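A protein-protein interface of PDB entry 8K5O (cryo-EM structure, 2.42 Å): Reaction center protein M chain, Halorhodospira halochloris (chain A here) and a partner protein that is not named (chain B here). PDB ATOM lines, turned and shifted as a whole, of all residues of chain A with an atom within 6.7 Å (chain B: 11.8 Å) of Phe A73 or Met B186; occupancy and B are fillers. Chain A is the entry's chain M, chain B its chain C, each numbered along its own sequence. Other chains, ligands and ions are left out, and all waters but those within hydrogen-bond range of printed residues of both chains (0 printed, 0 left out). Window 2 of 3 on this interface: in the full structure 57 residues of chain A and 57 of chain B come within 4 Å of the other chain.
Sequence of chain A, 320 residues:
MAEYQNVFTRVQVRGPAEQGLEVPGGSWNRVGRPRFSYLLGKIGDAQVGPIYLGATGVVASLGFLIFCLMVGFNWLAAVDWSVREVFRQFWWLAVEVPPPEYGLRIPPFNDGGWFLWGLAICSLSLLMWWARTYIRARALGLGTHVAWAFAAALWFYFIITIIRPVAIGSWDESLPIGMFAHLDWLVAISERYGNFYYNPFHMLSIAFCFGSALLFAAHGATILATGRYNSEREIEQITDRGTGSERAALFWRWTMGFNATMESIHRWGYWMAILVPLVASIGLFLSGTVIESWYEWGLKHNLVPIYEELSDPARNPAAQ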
ATOM      1  N   CYS A  68      -5.980 -12.343  19.113  1.00  0.00           N
ATOM      2  CA  CYS A  68      -6.193 -13.645  18.497  1.00  0.00           C
ATOM      3  C   CYS A  68      -4.884 -14.395  18.334  1.00  0.00           C
ATOM      4  O   CYS A  68      -4.832 -15.614  18.507  1.00  0.00           O
ATOM      5  CB  CYS A  68      -6.877 -13.474  17.141  1.00  0.00           C
ATOM      6  SG  CYS A  68      -8.617 -13.064  17.242  1.00  0.00           S
ATOM      7  N   LEU A  69      -3.817 -13.683  17.991  1.00  0.00           N
ATOM      8  CA  LEU A  69      -2.522 -14.321  17.820  1.00  0.00           C
ATOM      9  C   LEU A  69      -1.905 -14.693  19.161  1.00  0.00           C
ATOM     10  O   LEU A  69      -1.207 -15.702  19.259  1.00  0.00           O
ATOM     11  CB  LEU A  69      -1.609 -13.409  17.000  1.00  0.00           C
ATOM     12  CG  LEU A  69      -0.260 -13.968  16.564  1.00  0.00           C
ATOM     13  CD1 LEU A  69       0.221 -13.306  15.299  1.00  0.00           C
ATOM     14  CD2 LEU A  69       0.720 -13.685  17.665  1.00  0.00           C
ATOM     15  N   MET A  70      -2.146 -13.901  20.203  1.00  0.00           N
ATOM     16  CA  MET A  70      -1.743 -14.313  21.541  1.00  0.00           C
ATOM     17  C   MET A  70      -2.447 -15.598  21.933  1.00  0.00           C
ATOM     18  O   MET A  70      -1.826 -16.526  22.461  1.00  0.00           O
ATOM     19  CB  MET A  70      -2.052 -13.202  22.547  1.00  0.00           C
ATOM     20  CG  MET A  70      -1.582 -13.463  23.978  1.00  0.00           C
ATOM     21  SD  MET A  70      -2.603 -14.600  24.949  1.00  0.00           S
ATOM     22  CE  MET A  70      -4.150 -13.718  25.019  1.00  0.00           C
ATOM     23  N   VAL A  71      -3.750 -15.669  21.669  1.00  0.00           N
ATOM     24  CA  VAL A  71      -4.517 -16.867  21.980  1.00  0.00           C
ATOM     25  C   VAL A  71      -4.004 -18.050  21.172  1.00  0.00           C
ATOM     26  O   VAL A  71      -3.830 -19.151  21.701  1.00  0.00           O
ATOM     27  CB  VAL A  71      -6.013 -16.601  21.737  1.00  0.00           C
ATOM     28  CG1 VAL A  71      -6.803 -17.880  21.829  1.00  0.00           C
ATOM     29  CG2 VAL A  71      -6.526 -15.586  22.739  1.00  0.00           C
ATOM     30  N   GLY A  72      -3.730 -17.834  19.885  1.00  0.00           N
ATOM     31  CA  GLY A  72      -3.238 -18.911  19.045  1.00  0.00           C
ATOM     32  C   GLY A  72      -1.854 -19.386  19.436  1.00  0.00           C
ATOM     33  O   GLY A  72      -1.577 -20.586  19.416  1.00  0.00           O
ATOM     34  N   PHE A  73      -0.964 -18.457  19.784  1.00  0.00           N
ATOM     35  CA  PHE A  73       0.367 -18.827  20.243  1.00  0.00           C
ATOM     36  C   PHE A  73       0.307 -19.572  21.565  1.00  0.00           C
ATOM     37  O   PHE A  73       1.064 -20.522  21.780  1.00  0.00           O
ATOM     38  CB  PHE A  73       1.244 -17.582  20.365  1.00  0.00           C
ATOM     39  CG  PHE A  73       1.984 -17.240  19.109  1.00  0.00           C
ATOM     40  CD1 PHE A  73       1.313 -17.093  17.913  1.00  0.00           C
ATOM     41  CD2 PHE A  73       3.352 -17.060  19.126  1.00  0.00           C
ATOM     42  CE1 PHE A  73       1.992 -16.780  16.760  1.00  0.00           C
ATOM     43  CE2 PHE A  73       4.031 -16.748  17.975  1.00  0.00           C
ATOM     44  CZ  PHE A  73       3.351 -16.605  16.793  1.00  0.00           C
ATOM     45  N   ASN A  74      -0.585 -19.157  22.464  1.00  0.00           N
ATOM     46  CA  ASN A  74      -0.769 -19.905  23.701  1.00  0.00           C
ATOM     47  C   ASN A  74      -1.314 -21.298  23.426  1.00  0.00           C
ATOM     48  O   ASN A  74      -0.873 -22.270  24.038  1.00  0.00           O
ATOM     49  CB  ASN A  74      -1.684 -19.133  24.646  1.00  0.00           C
ATOM     50  CG  ASN A  74      -0.913 -18.244  25.588  1.00  0.00           C
ATOM     51  OD1 ASN A  74      -0.291 -18.722  26.531  1.00  0.00           O
ATOM     52  ND2 ASN A  74      -0.932 -16.946  25.329  1.00  0.00           N
ATOM     53  N   TRP A  75      -2.260 -21.422  22.498  1.00  0.00           N
ATOM     54  CA  TRP A  75      -2.780 -22.741  22.154  1.00  0.00           C
ATOM     55  C   TRP A  75      -1.685 -23.621  21.565  1.00  0.00           C
ATOM     56  O   TRP A  75      -1.568 -24.803  21.915  1.00  0.00           O
ATOM     57  CB  TRP A  75      -3.949 -22.602  21.184  1.00  0.00           C
ATOM     58  CG  TRP A  75      -5.152 -21.981  21.809  1.00  0.00           C
ATOM     59  CD1 TRP A  75      -5.241 -21.463  23.066  1.00  0.00           C
ATOM     60  CD2 TRP A  75      -6.443 -21.817  21.215  1.00  0.00           C
ATOM     61  NE1 TRP A  75      -6.501 -20.980  23.288  1.00  0.00           N
ATOM     62  CE2 TRP A  75      -7.261 -21.190  22.169  1.00  0.00           C
ATOM     63  CE3 TRP A  75      -6.986 -22.138  19.969  1.00  0.00           C
ATOM     64  CZ2 TRP A  75      -8.591 -20.872  21.916  1.00  0.00           C
ATOM     65  CZ3 TRP A  75      -8.306 -21.825  19.723  1.00  0.00           C
ATOM     66  CH2 TRP A  75      -9.094 -21.198  20.691  1.00  0.00           C
ATOM     67  N   LEU A  76      -0.862 -23.049  20.687  1.00  0.00           N
ATOM     68  CA  LEU A  76       0.262 -23.776  20.114  1.00  0.00           C
ATOM     69  C   LEU A  76       1.217 -24.249  21.200  1.00  0.00           C
ATOM     70  O   LEU A  76       1.544 -25.436  21.279  1.00  0.00           O
ATOM     71  CB  LEU A  76       0.991 -22.889  19.109  1.00  0.00           C
ATOM     72  CG  LEU A  76       0.291 -22.642  17.775  1.00  0.00           C
ATOM     73  CD1 LEU A  76       0.756 -21.332  17.157  1.00  0.00           C
ATOM     74  CD2 LEU A  76       0.541 -23.808  16.843  1.00  0.00           C
ATOM     75  N   ALA A  77       1.655 -23.331  22.063  1.00  0.00           N
ATOM     76  CA  ALA A  77       2.562 -23.700  23.143  1.00  0.00           C
ATOM     77  C   ALA A  77       1.918 -24.690  24.103  1.00  0.00           C
ATOM     78  O   ALA A  77       2.624 -25.432  24.795  1.00  0.00           O
ATOM     79  CB  ALA A  77       3.015 -22.446  23.887  1.00  0.00           C
ATOM     80  N   ALA A  78       0.588 -24.709  24.165  1.00  0.00           N
ATOM     81  CA  ALA A  78      -0.119 -25.680  24.984  1.00  0.00           C
ATOM     82  C   ALA A  78      -0.123 -27.058  24.347  1.00  0.00           C
ATOM     83  O   ALA A  78      -0.176 -28.066  25.060  1.00  0.00           O
ATOM     84  CB  ALA A  78      -1.553 -25.211  25.229  1.00  0.00           C
ATOM     85  N   TRP A  81       3.210 -26.593  20.101  1.00  0.00           N
ATOM     86  CA  TRP A  81       3.362 -25.840  18.856  1.00  0.00           C
ATOM     87  C   TRP A  81       2.966 -26.664  17.641  1.00  0.00           C
ATOM     88  O   TRP A  81       3.516 -26.497  16.552  1.00  0.00           O
ATOM     89  CB  TRP A  81       4.781 -25.298  18.722  1.00  0.00           C
ATOM     90  CG  TRP A  81       5.023 -24.231  19.721  1.00  0.00           C
ATOM     91  CD1 TRP A  81       5.492 -24.388  20.986  1.00  0.00           C
ATOM     92  CD2 TRP A  81       4.759 -22.838  19.559  1.00  0.00           C
ATOM     93  NE1 TRP A  81       5.560 -23.174  21.619  1.00  0.00           N
ATOM     94  CE2 TRP A  81       5.113 -22.205  20.762  1.00  0.00           C
ATOM     95  CE3 TRP A  81       4.271 -22.060  18.506  1.00  0.00           C
ATOM     96  CZ2 TRP A  81       4.992 -20.834  20.945  1.00  0.00           C
ATOM     97  CZ3 TRP A  81       4.149 -20.701  18.691  1.00  0.00           C
ATOM     98  CH2 TRP A  81       4.511 -20.102  19.901  1.00  0.00           C
ATOM     99  N   PHE A 109       2.643 -15.031  33.243  1.00  0.00           N
ATOM    100  CA  PHE A 109       1.931 -15.273  31.990  1.00  0.00           C
ATOM    101  C   PHE A 109       1.213 -16.613  31.981  1.00  0.00           C
ATOM    102  O   PHE A 109       0.026 -16.684  31.650  1.00  0.00           O
ATOM    103  CB  PHE A 109       2.878 -15.224  30.796  1.00  0.00           C
ATOM    104  CG  PHE A 109       3.269 -13.856  30.371  1.00  0.00           C
ATOM    105  CD1 PHE A 109       2.349 -13.030  29.759  1.00  0.00           C
ATOM    106  CD2 PHE A 109       4.579 -13.443  30.454  1.00  0.00           C
ATOM    107  CE1 PHE A 109       2.707 -11.791  29.318  1.00  0.00           C
ATOM    108  CE2 PHE A 109       4.944 -12.203  30.009  1.00  0.00           C
ATOM    109  CZ  PHE A 109       4.008 -11.381  29.434  1.00  0.00           C
ATOM    110  N   ASN A 110       1.931 -17.637  32.366  1.00  0.00           N
ATOM    111  CA  ASN A 110       1.378 -18.959  32.281  1.00  0.00           C
ATOM    112  C   ASN A 110       0.521 -19.367  33.480  1.00  0.00           C
ATOM    113  O   ASN A 110       0.002 -20.453  33.527  1.00  0.00           O
ATOM    114  CB  ASN A 110       2.522 -19.898  31.907  1.00  0.00           C
ATOM    115  CG  ASN A 110       2.431 -20.401  30.506  1.00  0.00           C
ATOM    116  OD1 ASN A 110       1.541 -20.026  29.765  1.00  0.00           O
ATOM    117  ND2 ASN A 110       3.330 -21.281  30.143  1.00  0.00           N
ATOM    118  N   TRP A 114      -1.244 -14.401  30.921  1.00  0.00           N
ATOM    119  CA  TRP A 114      -1.564 -14.251  29.508  1.00  0.00           C
ATOM    120  C   TRP A 114      -3.029 -13.906  29.324  1.00  0.00           C
ATOM    121  O   TRP A 114      -3.384 -13.132  28.432  1.00  0.00           O
ATOM    122  CB  TRP A 114      -1.227 -15.524  28.732  1.00  0.00           C
ATOM    123  CG  TRP A 114       0.158 -15.548  28.198  1.00  0.00           C
ATOM    124  CD1 TRP A 114       1.071 -16.536  28.360  1.00  0.00           C
ATOM    125  CD2 TRP A 114       0.793 -14.536  27.412  1.00  0.00           C
ATOM    126  NE1 TRP A 114       2.242 -16.208  27.732  1.00  0.00           N
ATOM    127  CE2 TRP A 114       2.098 -14.981  27.142  1.00  0.00           C
ATOM    128  CE3 TRP A 114       0.390 -13.290  26.921  1.00  0.00           C
ATOM    129  CZ2 TRP A 114       3.002 -14.232  26.398  1.00  0.00           C
ATOM    130  CZ3 TRP A 114       1.286 -12.550  26.182  1.00  0.00           C
ATOM    131  CH2 TRP A 114       2.577 -13.024  25.927  1.00  0.00           C
ATOM    132  N   GLU B 176       0.538 -32.828  33.041  1.00  0.00           N
ATOM    133  CA  GLU B 176       0.723 -31.397  33.235  1.00  0.00           C
ATOM    134  C   GLU B 176       0.873 -31.026  34.696  1.00  0.00           C
ATOM    135  O   GLU B 176       1.479 -29.992  34.994  1.00  0.00           O
ATOM    136  CB  GLU B 176      -0.453 -30.618  32.635  1.00  0.00           C
ATOM    137  CG  GLU B 176      -0.229 -29.120  32.532  1.00  0.00           C
ATOM    138  CD  GLU B 176      -1.490 -28.367  32.166  1.00  0.00           C
ATOM    139  OE1 GLU B 176      -2.198 -28.804  31.236  1.00  0.00           O
ATOM    140  OE2 GLU B 176      -1.771 -27.335  32.807  1.00  0.00           O
ATOM    141  N   GLU B 179       4.725 -31.926  35.247  1.00  0.00           N
ATOM    142  CA  GLU B 179       5.734 -31.233  34.461  1.00  0.00           C
ATOM    143  C   GLU B 179       6.203 -29.965  35.162  1.00  0.00           C
ATOM    144  O   GLU B 179       5.493 -29.366  35.974  1.00  0.00           O
ATOM    145  CB  GLU B 179       5.209 -30.862  33.075  1.00  0.00           C
ATOM    146  CG  GLU B 179       4.696 -32.009  32.244  1.00  0.00           C
ATOM    147  CD  GLU B 179       4.102 -31.531  30.938  1.00  0.00           C
ATOM    148  OE1 GLU B 179       3.618 -30.382  30.892  1.00  0.00           O
ATOM    149  OE2 GLU B 179       4.125 -32.300  29.955  1.00  0.00           O
ATOM    150  N   THR B 180       7.424 -29.559  34.833  1.00  0.00           N
ATOM    151  CA  THR B 180       7.924 -28.269  35.279  1.00  0.00           C
ATOM    152  C   THR B 180       7.181 -27.161  34.548  1.00  0.00           C
ATOM    153  O   THR B 180       7.091 -27.167  33.318  1.00  0.00           O
ATOM    154  CB  THR B 180       9.423 -28.159  35.022  1.00  0.00           C
ATOM    155  OG1 THR B 180      10.120 -29.122  35.822  1.00  0.00           O
ATOM    156  CG2 THR B 180       9.908 -26.777  35.372  1.00  0.00           C
ATOM    157  N   ARG B 181       6.646 -26.212  35.305  1.00  0.00           N
ATOM    158  CA  ARG B 181       5.830 -25.153  34.735  1.00  0.00           C
ATOM    159  C   ARG B 181       6.712 -24.000  34.281  1.00  0.00           C
ATOM    160  O   ARG B 181       7.541 -23.502  35.047  1.00  0.00           O
ATOM    161  CB  ARG B 181       4.800 -24.662  35.751  1.00  0.00           C
ATOM    162  CG  ARG B 181       3.594 -25.564  35.881  1.00  0.00           C
ATOM    163  CD  ARG B 181       2.526 -24.929  36.741  1.00  0.00           C
ATOM    164  NE  ARG B 181       1.736 -23.957  35.998  1.00  0.00           N
ATOM    165  CZ  ARG B 181       0.844 -23.143  36.545  1.00  0.00           C
ATOM    166  NH1 ARG B 181       0.617 -23.144  37.847  1.00  0.00           N
ATOM    167  NH2 ARG B 181       0.162 -22.312  35.765  1.00  0.00           N
ATOM    168  N   PHE B 182       6.538 -23.595  33.027  1.00  0.00           N
ATOM    169  CA  PHE B 182       7.169 -22.396  32.487  1.00  0.00           C
ATOM    170  C   PHE B 182       6.281 -21.221  32.864  1.00  0.00           C
ATOM    171  O   PHE B 182       5.369 -20.846  32.134  1.00  0.00           O
ATOM    172  CB  PHE B 182       7.342 -22.520  30.980  1.00  0.00           C
ATOM    173  CG  PHE B 182       8.251 -21.494  30.384  1.00  0.00           C
ATOM    174  CD1 PHE B 182       9.025 -20.681  31.186  1.00  0.00           C
ATOM    175  CD2 PHE B 182       8.334 -21.345  29.016  1.00  0.00           C
ATOM    176  CE1 PHE B 182       9.856 -19.741  30.629  1.00  0.00           C
ATOM    177  CE2 PHE B 182       9.167 -20.405  28.461  1.00  0.00           C
ATOM    178  CZ  PHE B 182       9.927 -19.604  29.266  1.00  0.00           C
ATOM    179  N   MET B 183       6.560 -20.622  34.021  1.00  0.00           N
ATOM    180  CA  MET B 183       5.611 -19.685  34.611  1.00  0.00           C
ATOM    181  C   MET B 183       5.474 -18.404  33.798  1.00  0.00           C
ATOM    182  O   MET B 183       4.398 -17.797  33.789  1.00  0.00           O
ATOM    183  CB  MET B 183       6.016 -19.371  36.047  1.00  0.00           C
ATOM    184  CG  MET B 183       5.892 -20.566  36.971  1.00  0.00           C
ATOM    185  SD  MET B 183       4.251 -21.300  36.948  1.00  0.00           S
ATOM    186  CE  MET B 183       3.271 -19.912  37.489  1.00  0.00           C
ATOM    187  N   THR B 184       6.530 -17.976  33.113  1.00  0.00           N
ATOM    188  CA  THR B 184       6.493 -16.737  32.353  1.00  0.00           C
ATOM    189  C   THR B 184       6.387 -17.003  30.846  1.00  0.00           C
ATOM    190  O   THR B 184       6.433 -16.068  30.045  1.00  0.00           O
ATOM    191  CB  THR B 184       7.731 -15.892  32.704  1.00  0.00           C
ATOM    192  OG1 THR B 184       7.724 -15.619  34.108  1.00  0.00           O
ATOM    193  CG2 THR B 184       7.694 -14.535  32.042  1.00  0.00           C
ATOM    194  N   GLY B 185       6.188 -18.248  30.448  1.00  0.00           N
ATOM    195  CA  GLY B 185       6.111 -18.610  29.046  1.00  0.00           C
ATOM    196  C   GLY B 185       4.707 -18.538  28.493  1.00  0.00           C
ATOM    197  O   GLY B 185       3.901 -17.688  28.883  1.00  0.00           O
ATOM    198  N   MET B 186       4.408 -19.445  27.567  1.00  0.00           N
ATOM    199  CA  MET B 186       3.103 -19.519  26.927  1.00  0.00           C
ATOM    200  C   MET B 186       2.562 -20.939  27.016  1.00  0.00           C
ATOM    201  O   MET B 186       3.287 -21.891  27.313  1.00  0.00           O
ATOM    202  CB  MET B 186       3.164 -19.094  25.455  1.00  0.00           C
ATOM    203  CG  MET B 186       3.637 -17.684  25.209  1.00  0.00           C
ATOM    204  SD  MET B 186       3.325 -17.190  23.513  1.00  0.00           S
ATOM    205  CE  MET B 186       1.864 -16.184  23.714  1.00  0.00           C
ATOM    206  N   GLY B 187       1.267 -21.069  26.749  1.00  0.00           N
ATOM    207  CA  GLY B 187       0.643 -22.367  26.612  1.00  0.00           C
ATOM    208  C   GLY B 187       0.511 -23.217  27.855  1.00  0.00           C
ATOM    209  O   GLY B 187       0.848 -24.403  27.833  1.00  0.00           O
ATOM    210  N   ASP B 188       0.028 -22.636  28.943  1.00  0.00           N
ATOM    211  CA  ASP B 188      -0.275 -23.382  30.156  1.00  0.00           C
ATOM    212  C   ASP B 188      -1.787 -23.386  30.322  1.00  0.00           C
ATOM    213  O   ASP B 188      -2.390 -22.349  30.613  1.00  0.00           O
ATOM    214  CB  ASP B 188       0.421 -22.769  31.364  1.00  0.00           C
ATOM    215  CG  ASP B 188       0.371 -23.657  32.584  1.00  0.00           C
ATOM    216  OD1 ASP B 188      -0.254 -24.735  32.529  1.00  0.00           O
ATOM    217  OD2 ASP B 188       0.983 -23.280  33.602  1.00  0.00           O
ATOM    218  N   LEU B 189      -2.391 -24.552  30.130  1.00  0.00           N
ATOM    219  CA  LEU B 189      -3.838 -24.688  30.193  1.00  0.00           C
ATOM    220  C   LEU B 189      -4.356 -24.801  31.617  1.00  0.00           C
ATOM    221  O   LEU B 189      -5.576 -24.828  31.810  1.00  0.00           O
ATOM    222  CB  LEU B 189      -4.277 -25.903  29.376  1.00  0.00           C
ATOM    223  CG  LEU B 189      -3.910 -25.875  27.892  1.00  0.00           C
ATOM    224  CD1 LEU B 189      -4.030 -27.256  27.290  1.00  0.00           C
ATOM    225  CD2 LEU B 189      -4.770 -24.886  27.130  1.00  0.00           C
ATOM    226  N   GLN B 190      -3.462 -24.852  32.606  1.00  0.00           N
ATOM    227  CA  GLN B 190      -3.829 -24.959  34.018  1.00  0.00           C
ATOM    228  C   GLN B 190      -4.674 -26.206  34.272  1.00  0.00           C
ATOM    229  O   GLN B 190      -5.688 -26.169  34.971  1.00  0.00           O
ATOM    230  CB  GLN B 190      -4.540 -23.693  34.498  1.00  0.00           C
ATOM    231  CG  GLN B 190      -3.747 -22.427  34.232  1.00  0.00           C
ATOM    232  CD  GLN B 190      -4.265 -21.238  35.004  1.00  0.00           C
ATOM    233  OE1 GLN B 190      -4.542 -21.331  36.195  1.00  0.00           O
ATOM    234  NE2 GLN B 190      -4.400 -20.108  34.326  1.00  0.00           N
ATOM    235  N   LEU B 191      -4.233 -27.322  33.688  1.00  0.00           N
ATOM    236  CA  LEU B 191      -4.887 -28.624  33.825  1.00  0.00           C
ATOM    237  C   LEU B 191      -6.319 -28.600  33.307  1.00  0.00           C
ATOM    238  O   LEU B 191      -7.136 -29.442  33.676  1.00  0.00           O
ATOM    239  CB  LEU B 191      -4.856 -29.128  35.273  1.00  0.00           C
ATOM    240  CG  LEU B 191      -3.622 -29.921  35.706  1.00  0.00           C
ATOM    241  CD1 LEU B 191      -3.480 -31.157  34.844  1.00  0.00           C
ATOM    242  CD2 LEU B 191      -2.362 -29.079  35.662  1.00  0.00           C
ATOM    243  N   ASN B 193      -8.903 -27.245  29.629  1.00  0.00           N
ATOM    244  CA  ASN B 193      -8.869 -26.807  28.237  1.00  0.00           C
ATOM    245  C   ASN B 193      -8.158 -27.811  27.340  1.00  0.00           C
ATOM    246  O   ASN B 193      -7.394 -27.452  26.443  1.00  0.00           O
ATOM    247  CB  ASN B 193      -8.217 -25.432  28.135  1.00  0.00           C
ATOM    248  CG  ASN B 193      -8.799 -24.448  29.117  1.00  0.00           C
ATOM    249  OD1 ASN B 193      -9.994 -24.170  29.094  1.00  0.00           O
ATOM    250  ND2 ASN B 193      -7.957 -23.909  29.983  1.00  0.00           N
ATOM    251  N   LYS B 194      -8.403 -29.091  27.590  1.00  0.00           N
ATOM    252  CA  LYS B 194      -7.821 -30.139  26.774  1.00  0.00           C
ATOM    253  C   LYS B 194      -8.761 -31.331  26.791  1.00  0.00           C
ATOM    254  O   LYS B 194      -9.531 -31.526  27.733  1.00  0.00           O
ATOM    255  CB  LYS B 194      -6.416 -30.518  27.266  1.00  0.00           C
ATOM    256  CG  LYS B 194      -5.681 -31.489  26.371  1.00  0.00           C
ATOM    257  CD  LYS B 194      -4.310 -31.848  26.907  1.00  0.00           C
ATOM    258  CE  LYS B 194      -3.338 -30.705  26.723  1.00  0.00           C
ATOM    259  NZ  LYS B 194      -3.055 -30.467  25.283  1.00  0.00           N
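Printed residues of chain B that touch a printed residue of chain A: Arg B181, Phe B182, Met B183, Thr B184, Gly B185, Met B186, Gly B187, Asp B188, Leu B189 and Lys B194.
Hydrophobic or aromatic side chains of chain B within 4 Å of the printed part of chain A: Met B186 and Leu B189.
Along chain B the printed residues that touch a printed residue of chain A span positions 181 to 194.
Hydrophobic or aromatic side chains of chain A that line the printed part of chain B: Phe A73, Ala A77, Ala A78, Phe A109 and Trp A114.
Among the printed residues, no Asp or Glu carboxylate lies within 4 Å of a Lys or Arg side-chain nitrogen of the other chain.
Among the printed residues, merely in contact across the chains: Met A70 with Met B186 (3.9 Å), Phe A73 with Met B186 (3.7 Å), Asn A74 with Met B186 (3.3 Å), Ala A77 with Met B186 (3.5 Å), Ala A77 with Gly B187 (3.6 Å), Ala A78 with Gly B187 (3.3 Å), Ala A78 with Leu B189 (3.6 Å), Ala A78 with Lys B194 (3.8 Å), Phe A109 with Thr B184 (3.2 Å), Phe A109 with Gly B185 (3.3 Å) and Trp A114 with Met B186 (3.2 Å).
The side-chain carboxylate (OD1) of Asp B188 sits close to the backbone NH (N) of Gln B190.
The backbone carbonyl oxygen (O) of Phe A109 sits at hydrogen-bond distance from the backbone NH (N) of Trp A114, at 2.7 Å.
NH2 of Arg B181 lies within salt-bridge range of OD2 of Asp B188, at 2.5 Å.
The side-chain sulfur of Met B183 sits close to the guanidinium group of Arg B181, 3.8 Å away.
The backbone carbonyl oxygen of Leu B189 is in hydrogen-bond range of the side-chain amide nitrogen of Asn B193, at 3.1 Å.
The side-chain sulfur (SD) of Met A70 sits at hydrogen-bond distance from the side-chain amide nitrogen (ND2) of Asn A74 (2.9 Å).
The backbone carbonyl oxygen of Met B183 sits at hydrogen-bond distance from the backbone NH of Phe A109, 3.3 Å away.
The backbone NH (N) of Asp B188 is in hydrogen-bond range of the side-chain amide oxygen (OD1) of Asn A110 (3.1 Å).
N of Asn A110 sits at hydrogen-bond distance from O of Met B183 (2.9 Å).
The indole nitrogen (NE1) of Trp A114 lies within hydrogen-bond range of the backbone carbonyl oxygen (O) of Gly B185 (2.5 Å).
The backbone NH (N) of Gly B187 lies within hydrogen-bond range of the side-chain amide oxygen (OD1) of Asn A110 (3.2 Å).
O of Met B186 sits at hydrogen-bond distance from ND2 of Asn A110, at 2.9 Å.
NH2 of Arg B181 sits at hydrogen-bond distance from O of Asn A110 (2.9 Å).
The backbone NH (N) of Gly B187 lies within hydrogen-bond range of the side-chain amide oxygen (OD1) of Asn A74, 2.8 Å away.
O of Phe B182 sits at hydrogen-bond distance from ND2 of Asn A110 (2.9 Å).
O of Gly B185 sits close to OD1 of Asn A110 (3.4 Å).
Phe A73 touches one residue of chain B.
Met B186 touches just these residues of chain A: Met A70, Phe A73, Asn A74, Ala A77, Asn A110 and Trp A114.
Met A70 touches just one residue of chain B: Met B186.
Val A71 touches none of the printed residues of chain B.
No residue of chain B comes within 4 Å of Gly A72.
Of chain B, only Met B186 (3.3 Å) and Gly B187 (2.8 Å) come within 4 Å of Asn A74.
No residue of chain B comes within 4 Å of Leu A76.
Of chain B, only Met B186 (3.5 Å) and Gly B187 (3.6 Å) come within 4 Å of Ala A77.
Printed residues of chain B within 4 Å of Trp A114: Gly B185 and Met B186.
Of the printed residues of chain A, Asp B188 touches Asn A110.
Of the printed residues of chain A, Met B183 touches Phe A109 (3.3 Å) and Asn A110 (2.9 Å).
Asn B193 touches none of the printed residues of chain A.
Glu B176 touches none of the printed residues of chain A.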
